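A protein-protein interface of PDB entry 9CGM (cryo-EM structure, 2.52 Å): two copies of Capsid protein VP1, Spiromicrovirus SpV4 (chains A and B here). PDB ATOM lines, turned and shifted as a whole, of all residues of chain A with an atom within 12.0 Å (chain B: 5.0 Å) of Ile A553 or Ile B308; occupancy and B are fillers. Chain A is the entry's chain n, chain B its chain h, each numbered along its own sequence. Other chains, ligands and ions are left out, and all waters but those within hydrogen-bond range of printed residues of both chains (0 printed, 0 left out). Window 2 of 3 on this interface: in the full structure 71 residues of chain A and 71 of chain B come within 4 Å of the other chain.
Printed residues of chain A that touch a printed residue of chain B: Gly A549, Leu A550, Arg A552 and Ile A553.
Among the printed residues, 7 pairs touch across the chains.
Among the printed residues, no Asp or Glu carboxylate lies within 4 Å of a Lys or Arg side-chain nitrogen of the other chain.
Arg B305 touches Gly A549.
CD1 of Leu A550 touches O of Arg B305, 3.9 Å away.
CD1 of Leu A550 touches CG2 of Ile B308, at 3.9 Å.
Leu A550 touches Thr B309.
CE1 of His B312 touches O of Arg A552, at 3.4 Å.
Ile A553 touches Ile B308.
NE2 of His B312 touches C of Ile A553, at 3.2 Å.
No position is printed for both chains.
Of the 7 pairs that touch across the chains among the printed residues, none has its exchanged pair printed and touching as well.
Of the printed residues of chain B, Gly A549 touches Arg B305 (3.9 Å).
Of the printed residues of chain B, Leu A550 touches Arg B305, Ile B308 and Thr B309.
Of the printed residues of chain B, Arg A552 touches His B312 (3.4 Å).
No residue of chain A comes within 4 Å of Leu B304.
No residue of chain A comes within 4 Å of Ala B307.
Ile B308 touches just these residues of chain A: Leu A550 (3.9 Å) and Ile A553 (3.3 Å).
Of chain A, only Leu A550 (3.9 Å) comes within 4 Å of Thr B309.
No residue of chain A comes within 4 Å of Gln B311.
His B312 touches two residues of chain A.
O of Leu B306 is in hydrogen-bond range of OG1 of Thr B309 (2.6 Å).
O of Arg B305 is in hydrogen-bond range of OG1 of Thr B309.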
ATOM      1  N   ASN A  21     -10.480  -2.975  18.907  1.00  0.00           N
ATOM      2  CA  ASN A  21     -10.120  -4.032  19.832  1.00  0.00           C
ATOM      3  C   ASN A  21      -8.769  -4.626  19.453  1.00  0.00           C
ATOM      4  O   ASN A  21      -8.139  -4.247  18.461  1.00  0.00           O
ATOM      5  CB  ASN A  21     -11.182  -5.128  19.840  1.00  0.00           C
ATOM      6  CG  ASN A  21     -12.479  -4.681  20.476  1.00  0.00           C
ATOM      7  OD1 ASN A  21     -12.509  -3.729  21.257  1.00  0.00           O
ATOM      8  ND2 ASN A  21     -13.560  -5.373  20.155  1.00  0.00           N
ATOM      9  N   PRO A 548     -15.323 -21.566  24.780  1.00  0.00           N
ATOM     10  CA  PRO A 548     -16.470 -20.723  25.118  1.00  0.00           C
ATOM     11  C   PRO A 548     -16.193 -19.795  26.293  1.00  0.00           C
ATOM     12  O   PRO A 548     -15.372 -20.076  27.165  1.00  0.00           O
ATOM     13  CB  PRO A 548     -17.560 -21.742  25.455  1.00  0.00           C
ATOM     14  CG  PRO A 548     -17.187 -22.926  24.680  1.00  0.00           C
ATOM     15  CD  PRO A 548     -15.698 -22.985  24.711  1.00  0.00           C
ATOM     16  N   GLY A 549     -16.919 -18.684  26.305  1.00  0.00           N
ATOM     17  CA  GLY A 549     -16.816 -17.614  27.282  1.00  0.00           C
ATOM     18  C   GLY A 549     -16.078 -16.397  26.770  1.00  0.00           C
ATOM     19  O   GLY A 549     -15.041 -16.514  26.119  1.00  0.00           O
ATOM     20  N   LEU A 550     -16.557 -15.221  27.147  1.00  0.00           N
ATOM     21  CA  LEU A 550     -16.171 -13.979  26.503  1.00  0.00           C
ATOM     22  C   LEU A 550     -15.368 -13.117  27.461  1.00  0.00           C
ATOM     23  O   LEU A 550     -15.534 -13.193  28.677  1.00  0.00           O
ATOM     24  CB  LEU A 550     -17.409 -13.216  26.040  1.00  0.00           C
ATOM     25  CG  LEU A 550     -18.358 -13.953  25.096  1.00  0.00           C
ATOM     26  CD1 LEU A 550     -19.631 -13.151  24.897  1.00  0.00           C
ATOM     27  CD2 LEU A 550     -17.693 -14.248  23.772  1.00  0.00           C
ATOM     28  N   ARG A 551     -14.485 -12.298  26.899  1.00  0.00           N
ATOM     29  CA  ARG A 551     -13.673 -11.400  27.701  1.00  0.00           C
ATOM     30  C   ARG A 551     -14.415 -10.144  28.124  1.00  0.00           C
ATOM     31  O   ARG A 551     -14.200  -9.661  29.239  1.00  0.00           O
ATOM     32  CB  ARG A 551     -12.419 -10.975  26.935  1.00  0.00           C
ATOM     33  CG  ARG A 551     -11.527 -12.077  26.389  1.00  0.00           C
ATOM     34  CD  ARG A 551     -10.859 -12.903  27.475  1.00  0.00           C
ATOM     35  NE  ARG A 551      -9.783 -13.725  26.923  1.00  0.00           N
ATOM     36  CZ  ARG A 551      -9.958 -14.899  26.327  1.00  0.00           C
ATOM     37  NH1 ARG A 551     -11.176 -15.385  26.163  1.00  0.00           N
ATOM     38  NH2 ARG A 551      -8.914 -15.567  25.858  1.00  0.00           N
ATOM     39  N   ARG A 552     -15.264  -9.604  27.260  1.00  0.00           N
ATOM     40  CA  ARG A 552     -15.984  -8.367  27.508  1.00  0.00           C
ATOM     41  C   ARG A 552     -17.467  -8.671  27.584  1.00  0.00           C
ATOM     42  O   ARG A 552     -17.936  -9.664  27.028  1.00  0.00           O
ATOM     43  CB  ARG A 552     -15.745  -7.347  26.400  1.00  0.00           C
ATOM     44  CG  ARG A 552     -14.306  -6.993  26.190  1.00  0.00           C
ATOM     45  CD  ARG A 552     -13.742  -6.186  27.331  1.00  0.00           C
ATOM     46  NE  ARG A 552     -12.332  -5.913  27.095  1.00  0.00           N
ATOM     47  CZ  ARG A 552     -11.888  -4.946  26.299  1.00  0.00           C
ATOM     48  NH1 ARG A 552     -12.747  -4.163  25.654  1.00  0.00           N
ATOM     49  NH2 ARG A 552     -10.586  -4.770  26.135  1.00  0.00           N
ATOM     50  N   ILE A 553     -18.205  -7.814  28.272  1.00  0.00           N
ATOM     51  CA  ILE A 553     -19.629  -8.039  28.394  1.00  0.00           C
ATOM     52  C   ILE A 553     -20.379  -6.978  27.606  1.00  0.00           C
ATOM     53  O   ILE A 553     -21.565  -7.129  27.319  1.00  0.00           O
ATOM     54  CB  ILE A 553     -20.074  -8.038  29.837  1.00  0.00           C
ATOM     55  CG1 ILE A 553     -21.355  -8.832  29.963  1.00  0.00           C
ATOM     56  CG2 ILE A 553     -20.414  -6.659  30.249  1.00  0.00           C
ATOM     57  CD1 ILE A 553     -21.137 -10.268  29.671  1.00  0.00           C
ATOM     58  N   LEU B 304     -27.364 -16.141  25.626  1.00  0.00           N
ATOM     59  CA  LEU B 304     -26.845 -14.917  26.213  1.00  0.00           C
ATOM     60  C   LEU B 304     -25.524 -14.520  25.571  1.00  0.00           C
ATOM     61  O   LEU B 304     -25.271 -13.337  25.336  1.00  0.00           O
ATOM     62  CB  LEU B 304     -26.682 -15.095  27.718  1.00  0.00           C
ATOM     63  CG  LEU B 304     -26.091 -13.911  28.476  1.00  0.00           C
ATOM     64  CD1 LEU B 304     -27.002 -12.710  28.374  1.00  0.00           C
ATOM     65  CD2 LEU B 304     -25.855 -14.282  29.914  1.00  0.00           C
ATOM     66  N   ARG B 305     -24.668 -15.495  25.281  1.00  0.00           N
ATOM     67  CA  ARG B 305     -23.399 -15.179  24.642  1.00  0.00           C
ATOM     68  C   ARG B 305     -23.597 -14.641  23.234  1.00  0.00           C
ATOM     69  O   ARG B 305     -22.884 -13.725  22.810  1.00  0.00           O
ATOM     70  CB  ARG B 305     -22.488 -16.405  24.630  1.00  0.00           C
ATOM     71  CG  ARG B 305     -21.756 -16.647  25.932  1.00  0.00           C
ATOM     72  CD  ARG B 305     -20.615 -17.620  25.715  1.00  0.00           C
ATOM     73  NE  ARG B 305     -21.077 -18.992  25.562  1.00  0.00           N
ATOM     74  CZ  ARG B 305     -21.100 -19.876  26.551  1.00  0.00           C
ATOM     75  NH1 ARG B 305     -20.630 -19.533  27.739  1.00  0.00           N
ATOM     76  NH2 ARG B 305     -21.548 -21.108  26.334  1.00  0.00           N
ATOM     77  N   LEU B 306     -24.548 -15.202  22.484  1.00  0.00           N
ATOM     78  CA  LEU B 306     -24.840 -14.674  21.157  1.00  0.00           C
ATOM     79  C   LEU B 306     -25.281 -13.226  21.216  1.00  0.00           C
ATOM     80  O   LEU B 306     -24.789 -12.392  20.451  1.00  0.00           O
ATOM     81  CB  LEU B 306     -25.911 -15.505  20.467  1.00  0.00           C
ATOM     82  CG  LEU B 306     -25.495 -16.837  19.880  1.00  0.00           C
ATOM     83  CD1 LEU B 306     -26.714 -17.571  19.402  1.00  0.00           C
ATOM     84  CD2 LEU B 306     -24.560 -16.564  18.731  1.00  0.00           C
ATOM     85  N   ALA B 307     -26.220 -12.910  22.106  1.00  0.00           N
ATOM     86  CA  ALA B 307     -26.741 -11.553  22.181  1.00  0.00           C
ATOM     87  C   ALA B 307     -25.642 -10.550  22.500  1.00  0.00           C
ATOM     88  O   ALA B 307     -25.608  -9.455  21.936  1.00  0.00           O
ATOM     89  CB  ALA B 307     -27.846 -11.489  23.227  1.00  0.00           C
ATOM     90  N   ILE B 308     -24.735 -10.912  23.399  1.00  0.00           N
ATOM     91  CA  ILE B 308     -23.658 -10.009  23.789  1.00  0.00           C
ATOM     92  C   ILE B 308     -22.722  -9.751  22.615  1.00  0.00           C
ATOM     93  O   ILE B 308     -22.229  -8.634  22.433  1.00  0.00           O
ATOM     94  CB  ILE B 308     -22.923 -10.595  25.006  1.00  0.00           C
ATOM     95  CG1 ILE B 308     -23.861 -10.616  26.205  1.00  0.00           C
ATOM     96  CG2 ILE B 308     -21.666  -9.818  25.327  1.00  0.00           C
ATOM     97  CD1 ILE B 308     -23.387 -11.480  27.316  1.00  0.00           C
ATOM     98  N   THR B 309     -22.482 -10.764  21.790  1.00  0.00           N
ATOM     99  CA  THR B 309     -21.614 -10.571  20.635  1.00  0.00           C
ATOM    100  C   THR B 309     -22.302  -9.758  19.550  1.00  0.00           C
ATOM    101  O   THR B 309     -21.640  -9.034  18.802  1.00  0.00           O
ATOM    102  CB  THR B 309     -21.161 -11.918  20.079  1.00  0.00           C
ATOM    103  OG1 THR B 309     -22.306 -12.723  19.789  1.00  0.00           O
ATOM    104  CG2 THR B 309     -20.268 -12.630  21.057  1.00  0.00           C
ATOM    105  N   TYR B 310     -23.623  -9.880  19.425  1.00  0.00           N
ATOM    106  CA  TYR B 310     -24.335  -9.045  18.467  1.00  0.00           C
ATOM    107  C   TYR B 310     -24.259  -7.579  18.856  1.00  0.00           C
ATOM    108  O   TYR B 310     -24.129  -6.706  17.994  1.00  0.00           O
ATOM    109  CB  TYR B 310     -25.792  -9.472  18.343  1.00  0.00           C
ATOM    110  CG  TYR B 310     -25.992 -10.835  17.742  1.00  0.00           C
ATOM    111  CD1 TYR B 310     -25.109 -11.334  16.808  1.00  0.00           C
ATOM    112  CD2 TYR B 310     -27.096 -11.596  18.066  1.00  0.00           C
ATOM    113  CE1 TYR B 310     -25.291 -12.571  16.248  1.00  0.00           C
ATOM    114  CE2 TYR B 310     -27.292 -12.831  17.502  1.00  0.00           C
ATOM    115  CZ  TYR B 310     -26.386 -13.310  16.590  1.00  0.00           C
ATOM    116  OH  TYR B 310     -26.578 -14.542  16.024  1.00  0.00           O
ATOM    117  N   GLN B 311     -24.345  -7.291  20.151  1.00  0.00           N
ATOM    118  CA  GLN B 311     -24.251  -5.917  20.619  1.00  0.00           C
ATOM    119  C   GLN B 311     -22.841  -5.376  20.438  1.00  0.00           C
ATOM    120  O   GLN B 311     -22.660  -4.219  20.054  1.00  0.00           O
ATOM    121  CB  GLN B 311     -24.694  -5.855  22.080  1.00  0.00           C
ATOM    122  CG  GLN B 311     -24.776  -4.480  22.715  1.00  0.00           C
ATOM    123  CD  GLN B 311     -25.789  -3.581  22.056  1.00  0.00           C
ATOM    124  OE1 GLN B 311     -26.930  -3.970  21.844  1.00  0.00           O
ATOM    125  NE2 GLN B 311     -25.397  -2.349  21.788  1.00  0.00           N
ATOM    126  N   HIS B 312     -21.828  -6.202  20.697  1.00  0.00           N
ATOM    127  CA  HIS B 312     -20.457  -5.792  20.423  1.00  0.00           C
ATOM    128  C   HIS B 312     -20.251  -5.508  18.950  1.00  0.00           C
ATOM    129  O   HIS B 312     -19.473  -4.624  18.580  1.00  0.00           O
ATOM    130  CB  HIS B 312     -19.481  -6.866  20.883  1.00  0.00           C
ATOM    131  CG  HIS B 312     -19.368  -6.981  22.365  1.00  0.00           C
ATOM    132  ND1 HIS B 312     -18.816  -8.078  22.985  1.00  0.00           N
ATOM    133  CD2 HIS B 312     -19.705  -6.119  23.351  1.00  0.00           C
ATOM    134  CE1 HIS B 312     -18.832  -7.894  24.290  1.00  0.00           C
ATOM    135  NE2 HIS B 312     -19.363  -6.713  24.539  1.00  0.00           N
